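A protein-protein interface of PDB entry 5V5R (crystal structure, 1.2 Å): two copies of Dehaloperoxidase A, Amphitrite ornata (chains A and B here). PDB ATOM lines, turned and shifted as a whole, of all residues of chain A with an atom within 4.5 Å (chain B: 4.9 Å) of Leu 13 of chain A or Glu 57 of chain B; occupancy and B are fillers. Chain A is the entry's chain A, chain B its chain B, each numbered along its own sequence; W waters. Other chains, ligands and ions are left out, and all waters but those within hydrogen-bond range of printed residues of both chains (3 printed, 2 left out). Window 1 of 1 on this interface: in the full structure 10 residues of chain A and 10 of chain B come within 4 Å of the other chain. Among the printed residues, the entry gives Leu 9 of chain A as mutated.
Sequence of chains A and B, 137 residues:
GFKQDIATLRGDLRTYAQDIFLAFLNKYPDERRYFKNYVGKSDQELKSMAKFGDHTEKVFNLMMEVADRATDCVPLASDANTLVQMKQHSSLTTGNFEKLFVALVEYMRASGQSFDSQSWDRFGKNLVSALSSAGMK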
ATOM      1  N   LEU A   9      22.928  19.498  32.084  1.00  0.00           N
ATOM      2  CA  LEU A   9      21.642  19.525  31.400  1.00  0.00           C
ATOM      3  C   LEU A   9      21.226  18.133  30.946  1.00  0.00           C
ATOM      4  O   LEU A   9      20.090  17.730  31.155  1.00  0.00           O
ATOM      5  CB  LEU A   9      21.698  20.518  30.220  1.00  0.00           C
ATOM      6  CG  LEU A   9      21.897  21.990  30.634  1.00  0.00           C
ATOM      7  CD1 LEU A   9      22.245  22.826  29.416  1.00  0.00           C
ATOM      8  CD2 LEU A   9      20.649  22.530  31.323  1.00  0.00           C
ATOM      9  N   ARG A  10      22.165  17.374  30.367  1.00  0.00           N
ATOM     10  CA  ARG A  10      21.842  16.038  29.868  1.00  0.00           C
ATOM     11  C   ARG A  10      21.413  15.119  30.992  1.00  0.00           C
ATOM     12  O   ARG A  10      20.654  14.161  30.765  1.00  0.00           O
ATOM     13  CB  ARG A  10      23.061  15.445  29.166  1.00  0.00           C
ATOM     14  CG  ARG A  10      23.227  15.942  27.735  1.00  0.00           C
ATOM     15  CD  ARG A  10      24.509  15.378  27.131  1.00  0.00           C
ATOM     16  NE  ARG A  10      24.518  15.582  25.696  1.00  0.00           N
ATOM     17  CZ  ARG A  10      25.591  15.535  24.932  1.00  0.00           C
ATOM     18  NH1 ARG A  10      26.804  15.364  25.458  1.00  0.00           N
ATOM     19  NH2 ARG A  10      25.424  15.632  23.605  1.00  0.00           N
ATOM     20  N   GLY A  11      21.898  15.355  32.208  1.00  0.00           N
ATOM     21  CA  GLY A  11      21.574  14.493  33.355  1.00  0.00           C
ATOM     22  C   GLY A  11      20.155  14.635  33.849  1.00  0.00           C
ATOM     23  O   GLY A  11      19.697  13.790  34.625  1.00  0.00           O
ATOM     24  N   ASP A  12      19.456  15.690  33.452  1.00  0.00           N
ATOM     25  CA  ASP A  12      18.058  15.859  33.812  1.00  0.00           C
ATOM     26  C   ASP A  12      17.349  16.572  32.663  1.00  0.00           C
ATOM     27  O   ASP A  12      16.688  17.600  32.852  1.00  0.00           O
ATOM     28  CB  ASP A  12      17.922  16.619  35.129  1.00  0.00           C
ATOM     29  CG  ASP A  12      16.591  16.394  35.790  1.00  0.00           C
ATOM     30  OD1 ASP A  12      15.861  15.447  35.452  1.00  0.00           O
ATOM     31  OD2 ASP A  12      16.287  17.164  36.714  1.00  0.00           O
ATOM     32  N   LEU A  13      17.471  16.009  31.446  1.00  0.00           N
ATOM     33  CA  LEU A  13      17.227  16.777  30.231  1.00  0.00           C
ATOM     34  C   LEU A  13      15.764  17.103  30.054  1.00  0.00           C
ATOM     35  O   LEU A  13      15.440  18.221  29.639  1.00  0.00           O
ATOM     36  CB  LEU A  13      17.808  16.058  29.017  1.00  0.00           C
ATOM     37  CG  LEU A  13      17.856  17.019  27.800  1.00  0.00           C
ATOM     38  CD1 LEU A  13      18.711  18.225  28.115  1.00  0.00           C
ATOM     39  CD2 LEU A  13      18.433  16.293  26.669  1.00  0.00           C
ATOM     40  N   ARG A  14      14.857  16.169  30.347  1.00  0.00           N
ATOM     41  CA  ARG A  14      13.453  16.487  30.114  1.00  0.00           C
ATOM     42  C   ARG A  14      13.013  17.640  30.994  1.00  0.00           C
ATOM     43  O   ARG A  14      12.309  18.536  30.511  1.00  0.00           O
ATOM     44  CB  ARG A  14      12.569  15.268  30.349  1.00  0.00           C
ATOM     45  CG  ARG A  14      11.116  15.463  29.880  1.00  0.00           C
ATOM     46  CD  ARG A  14      10.355  14.145  29.993  1.00  0.00           C
ATOM     47  NE  ARG A  14       9.004  14.205  29.435  1.00  0.00           N
ATOM     48  CZ  ARG A  14       8.694  13.990  28.154  1.00  0.00           C
ATOM     49  NH1 ARG A  14       9.649  13.764  27.269  1.00  0.00           N
ATOM     50  NH2 ARG A  14       7.429  14.031  27.755  1.00  0.00           N
ATOM     51  N   THR A  15      13.451  17.654  32.257  1.00  0.00           N
ATOM     52  CA  THR A  15      13.097  18.748  33.149  1.00  0.00           C
ATOM     53  C   THR A  15      13.692  20.074  32.681  1.00  0.00           C
ATOM     54  O   THR A  15      12.993  21.101  32.616  1.00  0.00           O
ATOM     55  CB  THR A  15      13.526  18.415  34.559  1.00  0.00           C
ATOM     56  OG1 THR A  15      12.888  17.166  34.894  1.00  0.00           O
ATOM     57  CG2 THR A  15      13.043  19.501  35.492  1.00  0.00           C
ATOM     58  N   TYR A  16      14.996  20.079  32.416  1.00  0.00           N
ATOM     59  CA  TYR A  16      15.632  21.324  31.998  1.00  0.00           C
ATOM     60  C   TYR A  16      15.091  21.812  30.660  1.00  0.00           C
ATOM     61  O   TYR A  16      14.914  23.033  30.464  1.00  0.00           O
ATOM     62  CB  TYR A  16      17.141  21.150  31.904  1.00  0.00           C
ATOM     63  CG  TYR A  16      17.883  21.190  33.227  1.00  0.00           C
ATOM     64  CD1 TYR A  16      17.830  22.332  34.037  1.00  0.00           C
ATOM     65  CD2 TYR A  16      18.725  20.136  33.619  1.00  0.00           C
ATOM     66  CE1 TYR A  16      18.538  22.383  35.227  1.00  0.00           C
ATOM     67  CE2 TYR A  16      19.437  20.174  34.789  1.00  0.00           C
ATOM     68  CZ  TYR A  16      19.341  21.278  35.601  1.00  0.00           C
ATOM     69  OH  TYR A  16      20.058  21.381  36.781  1.00  0.00           O
ATOM     70  N   ALA A  17      14.912  20.907  29.697  1.00  0.00           N
ATOM     71  CA  ALA A  17      14.415  21.310  28.384  1.00  0.00           C
ATOM     72  C   ALA A  17      13.040  21.952  28.497  1.00  0.00           C
ATOM     73  O   ALA A  17      12.781  23.012  27.908  1.00  0.00           O
ATOM     74  CB  ALA A  17      14.363  20.110  27.458  1.00  0.00           C
ATOM     75  N   GLU A  57      12.567  17.789  24.282  1.00  0.00           N
ATOM     76  CA  GLU A  57      13.718  16.919  24.443  1.00  0.00           C
ATOM     77  C   GLU A  57      14.450  16.710  23.128  1.00  0.00           C
ATOM     78  O   GLU A  57      15.679  16.658  23.111  1.00  0.00           O
ATOM     79  CB  GLU A  57      13.312  15.607  25.075  1.00  0.00           C
ATOM     80  CG  GLU A  57      13.019  15.765  26.502  1.00  0.00           C
ATOM     81  CD  GLU A  57      13.352  14.479  27.166  1.00  0.00           C
ATOM     82  OE1 GLU A  57      14.491  14.360  27.692  1.00  0.00           O
ATOM     83  OE2 GLU A  57      12.512  13.555  27.061  1.00  0.00           O
ATOM     84  N   PHE A  60      16.478  19.889  22.635  1.00  0.00           N
ATOM     85  CA  PHE A  60      17.624  19.975  23.532  1.00  0.00           C
ATOM     86  C   PHE A  60      18.623  18.855  23.307  1.00  0.00           C
ATOM     87  O   PHE A  60      19.822  19.065  23.490  1.00  0.00           O
ATOM     88  CB  PHE A  60      17.186  20.187  24.992  1.00  0.00           C
ATOM     89  CG  PHE A  60      16.848  21.628  25.269  1.00  0.00           C
ATOM     90  CD1 PHE A  60      17.737  22.478  25.907  1.00  0.00           C
ATOM     91  CD2 PHE A  60      15.658  22.153  24.798  1.00  0.00           C
ATOM     92  CE1 PHE A  60      17.417  23.826  26.134  1.00  0.00           C
ATOM     93  CE2 PHE A  60      15.332  23.522  24.988  1.00  0.00           C
ATOM     94  CZ  PHE A  60      16.214  24.333  25.650  1.00  0.00           C
ATOM     95  N   ASN A  61      18.170  17.665  22.883  1.00  0.00           N
ATOM     96  CA  ASN A  61      19.135  16.634  22.517  1.00  0.00           C
ATOM     97  C   ASN A  61      20.061  17.171  21.438  1.00  0.00           C
ATOM     98  O   ASN A  61      21.288  17.017  21.509  1.00  0.00           O
ATOM     99  CB  ASN A  61      18.406  15.423  21.929  1.00  0.00           C
ATOM    100  CG  ASN A  61      17.656  14.598  22.946  1.00  0.00           C
ATOM    101  OD1 ASN A  61      17.967  14.606  24.124  1.00  0.00           O
ATOM    102  ND2 ASN A  61      16.714  13.768  22.445  1.00  0.00           N
ATOM    103  N   MET A  64      22.346  20.108  22.637  1.00  0.00           N
ATOM    104  CA  MET A  64      23.481  19.659  23.433  1.00  0.00           C
ATOM    105  C   MET A  64      24.543  19.020  22.557  1.00  0.00           C
ATOM    106  O   MET A  64      25.741  19.161  22.841  1.00  0.00           O
ATOM    107  CB  MET A  64      23.064  18.716  24.587  1.00  0.00           C
ATOM    108  CG  MET A  64      22.161  19.358  25.653  1.00  0.00           C
ATOM    109  SD  MET A  64      22.934  20.774  26.453  1.00  0.00           S
ATOM    110  CE  MET A  64      22.149  22.128  25.564  1.00  0.00           C
ATOM    111  N   LEU B  13      17.067  10.245  22.240  1.00  0.00           N
ATOM    112  CA  LEU B  13      17.533   9.367  23.303  1.00  0.00           C
ATOM    113  C   LEU B  13      16.385   8.699  24.032  1.00  0.00           C
ATOM    114  O   LEU B  13      16.463   7.502  24.331  1.00  0.00           O
ATOM    115  CB  LEU B  13      18.443  10.135  24.245  1.00  0.00           C
ATOM    116  CG  LEU B  13      19.230   9.236  25.217  1.00  0.00           C
ATOM    117  CD1 LEU B  13      20.177   8.282  24.499  1.00  0.00           C
ATOM    118  CD2 LEU B  13      20.002  10.123  26.185  1.00  0.00           C
ATOM    119  N   ARG B  14      15.324   9.418  24.356  1.00  0.00           N
ATOM    120  CA  ARG B  14      14.236   8.810  25.132  1.00  0.00           C
ATOM    121  C   ARG B  14      13.596   7.651  24.368  1.00  0.00           C
ATOM    122  O   ARG B  14      13.260   6.589  24.936  1.00  0.00           O
ATOM    123  CB  ARG B  14      13.203   9.897  25.437  1.00  0.00           C
ATOM    124  CG  ARG B  14      12.160   9.546  26.484  1.00  0.00           C
ATOM    125  CD  ARG B  14      11.359  10.802  26.895  1.00  0.00           C
ATOM    126  NE  ARG B  14      10.390  10.589  27.971  1.00  0.00           N
ATOM    127  CZ  ARG B  14      10.663  10.756  29.261  1.00  0.00           C
ATOM    128  NH1 ARG B  14      11.898  11.078  29.630  1.00  0.00           N
ATOM    129  NH2 ARG B  14       9.715  10.581  30.184  1.00  0.00           N
ATOM    130  N   ALA B  17      16.132   4.735  24.156  1.00  0.00           N
ATOM    131  CA  ALA B  17      16.348   4.174  25.477  1.00  0.00           C
ATOM    132  C   ALA B  17      15.170   3.280  25.867  1.00  0.00           C
ATOM    133  O   ALA B  17      15.363   2.152  26.375  1.00  0.00           O
ATOM    134  CB  ALA B  17      16.503   5.283  26.504  1.00  0.00           C
ATOM    135  N   PHE B  52       9.477   5.565  34.453  1.00  0.00           N
ATOM    136  CA  PHE B  52       9.948   4.726  33.334  1.00  0.00           C
ATOM    137  C   PHE B  52      10.734   5.519  32.286  1.00  0.00           C
ATOM    138  O   PHE B  52      11.862   5.172  31.942  1.00  0.00           O
ATOM    139  CB  PHE B  52       8.797   3.953  32.657  1.00  0.00           C
ATOM    140  CG  PHE B  52       9.259   3.072  31.516  1.00  0.00           C
ATOM    141  CD1 PHE B  52       9.883   1.857  31.770  1.00  0.00           C
ATOM    142  CD2 PHE B  52       9.144   3.466  30.179  1.00  0.00           C
ATOM    143  CE1 PHE B  52      10.363   1.047  30.712  1.00  0.00           C
ATOM    144  CE2 PHE B  52       9.591   2.673  29.146  1.00  0.00           C
ATOM    145  CZ  PHE B  52      10.225   1.451  29.409  1.00  0.00           C
ATOM    146  N   GLY B  53      10.143   6.570  31.725  1.00  0.00           N
ATOM    147  CA  GLY B  53      10.890   7.353  30.759  1.00  0.00           C
ATOM    148  C   GLY B  53      12.089   8.045  31.392  1.00  0.00           C
ATOM    149  O   GLY B  53      13.170   8.105  30.797  1.00  0.00           O
ATOM    150  N   ASP B  54      11.940   8.497  32.644  1.00  0.00           N
ATOM    151  CA  ASP B  54      13.079   9.146  33.288  1.00  0.00           C
ATOM    152  C   ASP B  54      14.197   8.142  33.597  1.00  0.00           C
ATOM    153  O   ASP B  54      15.388   8.438  33.368  1.00  0.00           O
ATOM    154  CB  ASP B  54      12.619   9.865  34.544  1.00  0.00           C
ATOM    155  CG  ASP B  54      11.744  11.069  34.238  1.00  0.00           C
ATOM    156  OD1 ASP B  54      11.671  11.483  33.057  1.00  0.00           O
ATOM    157  OD2 ASP B  54      11.106  11.557  35.182  1.00  0.00           O
ATOM    158  N   HIS B  55      13.842   6.942  34.085  1.00  0.00           N
ATOM    159  CA  HIS B  55      14.858   5.934  34.324  1.00  0.00           C
ATOM    160  C   HIS B  55      15.588   5.616  33.038  1.00  0.00           C
ATOM    161  O   HIS B  55      16.828   5.657  32.981  1.00  0.00           O
ATOM    162  CB  HIS B  55      14.205   4.662  34.885  1.00  0.00           C
ATOM    163  CG  HIS B  55      15.146   3.511  34.938  1.00  0.00           C
ATOM    164  ND1 HIS B  55      16.134   3.424  35.897  1.00  0.00           N
ATOM    165  CD2 HIS B  55      15.353   2.479  34.091  1.00  0.00           C
ATOM    166  CE1 HIS B  55      16.878   2.356  35.673  1.00  0.00           C
ATOM    167  NE2 HIS B  55      16.442   1.785  34.565  1.00  0.00           N
ATOM    168  N   THR B  56      14.838   5.254  31.990  1.00  0.00           N
ATOM    169  CA  THR B  56      15.498   4.757  30.788  1.00  0.00           C
ATOM    170  C   THR B  56      16.366   5.845  30.165  1.00  0.00           C
ATOM    171  O   THR B  56      17.487   5.583  29.712  1.00  0.00           O
ATOM    172  CB  THR B  56      14.505   4.142  29.780  1.00  0.00           C
ATOM    173  OG1 THR B  56      13.505   5.097  29.434  1.00  0.00           O
ATOM    174  CG2 THR B  56      13.860   2.894  30.345  1.00  0.00           C
ATOM    175  N   GLU B  57      15.862   7.087  30.117  1.00  0.00           N
ATOM    176  CA  GLU B  57      16.653   8.137  29.503  1.00  0.00           C
ATOM    177  C   GLU B  57      17.929   8.373  30.291  1.00  0.00           C
ATOM    178  O   GLU B  57      19.002   8.532  29.691  1.00  0.00           O
ATOM    179  CB  GLU B  57      15.853   9.422  29.391  1.00  0.00           C
ATOM    180  CG  GLU B  57      16.744  10.503  28.786  1.00  0.00           C
ATOM    181  CD  GLU B  57      16.091  11.844  28.687  1.00  0.00           C
ATOM    182  OE1 GLU B  57      16.889  12.829  28.625  1.00  0.00           O
ATOM    183  OE2 GLU B  57      14.835  11.917  28.648  1.00  0.00           O
ATOM    184  N   LYS B  58      17.834   8.410  31.636  1.00  0.00           N
ATOM    185  CA  LYS B  58      19.032   8.677  32.443  1.00  0.00           C
ATOM    186  C   LYS B  58      20.051   7.561  32.343  1.00  0.00           C
ATOM    187  O   LYS B  58      21.258   7.816  32.329  1.00  0.00           O
ATOM    188  CB  LYS B  58      18.635   8.992  33.868  1.00  0.00           C
ATOM    189  CG  LYS B  58      17.897  10.380  33.918  1.00  0.00           C
ATOM    190  CD  LYS B  58      17.349  10.678  35.274  1.00  0.00           C
ATOM    191  CE  LYS B  58      16.618  12.053  35.305  1.00  0.00           C
ATOM    192  NZ  LYS B  58      15.946  12.280  36.604  1.00  0.00           N
ATOM    193  N   VAL B  59      19.582   6.317  32.273  1.00  0.00           N
ATOM    194  CA  VAL B  59      20.486   5.187  32.057  1.00  0.00           C
ATOM    195  C   VAL B  59      21.219   5.367  30.745  1.00  0.00           C
ATOM    196  O   VAL B  59      22.440   5.249  30.668  1.00  0.00           O
ATOM    197  CB  VAL B  59      19.642   3.899  32.007  1.00  0.00           C
ATOM    198  CG1 VAL B  59      20.475   2.718  31.452  1.00  0.00           C
ATOM    199  CG2 VAL B  59      19.122   3.589  33.421  1.00  0.00           C
ATOM    200  N   PHE B  60      20.480   5.642  29.670  1.00  0.00           N
ATOM    201  CA  PHE B  60      21.128   5.727  28.369  1.00  0.00           C
ATOM    202  C   PHE B  60      21.960   6.980  28.227  1.00  0.00           C
ATOM    203  O   PHE B  60      22.963   6.974  27.488  1.00  0.00           O
ATOM    204  CB  PHE B  60      20.108   5.519  27.233  1.00  0.00           C
ATOM    205  CG  PHE B  60      19.823   4.053  27.007  1.00  0.00           C
ATOM    206  CD1 PHE B  60      20.444   3.364  25.990  1.00  0.00           C
ATOM    207  CD2 PHE B  60      19.054   3.334  27.913  1.00  0.00           C
ATOM    208  CE1 PHE B  60      20.247   2.003  25.818  1.00  0.00           C
ATOM    209  CE2 PHE B  60      18.857   1.936  27.786  1.00  0.00           C
ATOM    210  CZ  PHE B  60      19.463   1.286  26.736  1.00  0.00           C
ATOM    211  N   ASN B  61      21.581   8.087  28.901  1.00  0.00           N
ATOM    212  CA  ASN B  61      22.477   9.235  28.922  1.00  0.00           C
ATOM    213  C   ASN B  61      23.834   8.850  29.521  1.00  0.00           C
ATOM    214  O   ASN B  61      24.894   9.175  28.981  1.00  0.00           O
ATOM    215  CB  ASN B  61      21.858  10.379  29.689  1.00  0.00           C
ATOM    216  CG  ASN B  61      22.825  11.506  29.808  1.00  0.00           C
ATOM    217  OD1 ASN B  61      23.270  12.090  28.796  1.00  0.00           O
ATOM    218  ND2 ASN B  61      23.220  11.802  31.042  1.00  0.00           N
HETATM  219  O   HOH W   1      18.627  13.686  37.495  1.00  0.00           O
HETATM  220  O   HOH W   2      18.179  13.144  31.384  1.00  0.00           O
HETATM  221  O   HOH W   3      15.317  13.221  31.374  1.00  0.00           O
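OE1 of Glu 57 of chain A lies close to OE2 of Glu 57 of chain B (2.6 Å). The backbone carbonyl oxygen (O) of Arg 10 of chain A lies within hydrogen-bond range of the side-chain amide nitrogen (ND2) of Asn 61 of chain B (3.5 Å). The guanidinium group of Arg 14 of chain B is in salt-bridge range of the side-chain carboxylate of Glu 57 of chain A (3.6 Å). NE of Arg 14 of chain B sits close to NH1 of Arg 14 of chain A. OD1 of Asp 12 of chain A lies within salt-bridge range of NZ of Lys 58 of chain B (3.4 Å).
OD1 of Asp 54 of chain B lies within salt-bridge range of NH1 of Arg 14 of chain B (3.5 Å). The backbone carbonyl oxygen (O) of Glu 57 of chain A sits close to the side-chain amide nitrogen (ND2) of Asn 61 of chain A (3.1 Å). The guanidinium group (NH1) of Arg 14 of chain B is in hydrogen-bond range of the backbone carbonyl oxygen (O) of Gly 53 of chain B. The guanidinium group (NH1) of Arg 14 of chain A lies within salt-bridge range of the side-chain carboxylate (OE2) of Glu 57 of chain A. OE2 of Glu 57 of chain B is in salt-bridge range of NH1 of Arg 14 of chain B, 3.2 Å away. The side-chain hydroxyl (OG1) of Thr 15 of chain A sits at hydrogen-bond distance from the side-chain carboxylate (OD1) of Asp 12 of chain A, at 3.5 Å.
Gly 11 of chain A touches Lys 58 of chain B (O to CE, 3.6 Å). ND2 of Asn 61 of chain B touches CA of Gly 11 of chain A (3.9 Å). Glu 57 of chain B touches Leu 13 of chain A. Asn 61 of chain A touches Leu 13 of chain B.
Of the printed residues of chain B, Asp 12 of chain A touches Lys 58. Of the printed residues of chain B, Leu 13 of chain A touches Glu 57. Of the printed residues of chain B, Arg 14 of chain A touches Arg 14. Printed residues of chain B within 4 Å of Glu 57 of chain A: Arg 14 and Glu 57. Of the printed residues of chain A, Arg 14 of chain B touches Arg 14 and Glu 57. Of the printed residues of chain A, Glu 57 of chain B touches Leu 13 (3.4 Å) and Glu 57 (2.6 Å). The nearest printed residue of chain B that does not touch Leu 13 of chain A is Lys 58 of chain B (5.6 Å).
Of the 13 printed residues of chain A, 7 touch a printed residue of chain B. Hydrophobic or aromatic side chains of chain A that line the printed part of chain B: Leu 13. Along chain A the printed residues that touch a printed residue of chain B span positions 10 to 61. Along chain B the printed residues that touch a printed residue of chain A span positions 13 to 61.
Arg 14 of chain B touches its own counterpart, Arg 14 of chain A. Glu 57 of chain A touches Arg 14 of chain B, but with the chains exchanged Arg 14 of chain A does not touch Glu 57 of chain B (4.3 Å). Glu 57 of chain B touches its own counterpart, Glu 57 of chain A. Asn 61 of chain A touches Leu 13 of chain B, but with the chains exchanged Leu 13 of chain A does not touch Asn 61 of chain B (6.8 Å). 6 positions are printed for both chains.
Water W2 lies within hydrogen-bond range of the backbone carbonyl oxygen (O) of Arg 10 of chain A, the backbone NH (N) of Leu 13 of chain A and the side-chain carboxylate (OE1) of Glu 57 of chain B. Water W3 bridges OE2 of Glu 57 of chain B and N of Arg 14 of chain A. Water W1 lies within hydrogen-bond range of O of Gly 11 of chain A (3.1 Å) and NZ of Lys 58 of chain B (3.2 Å).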
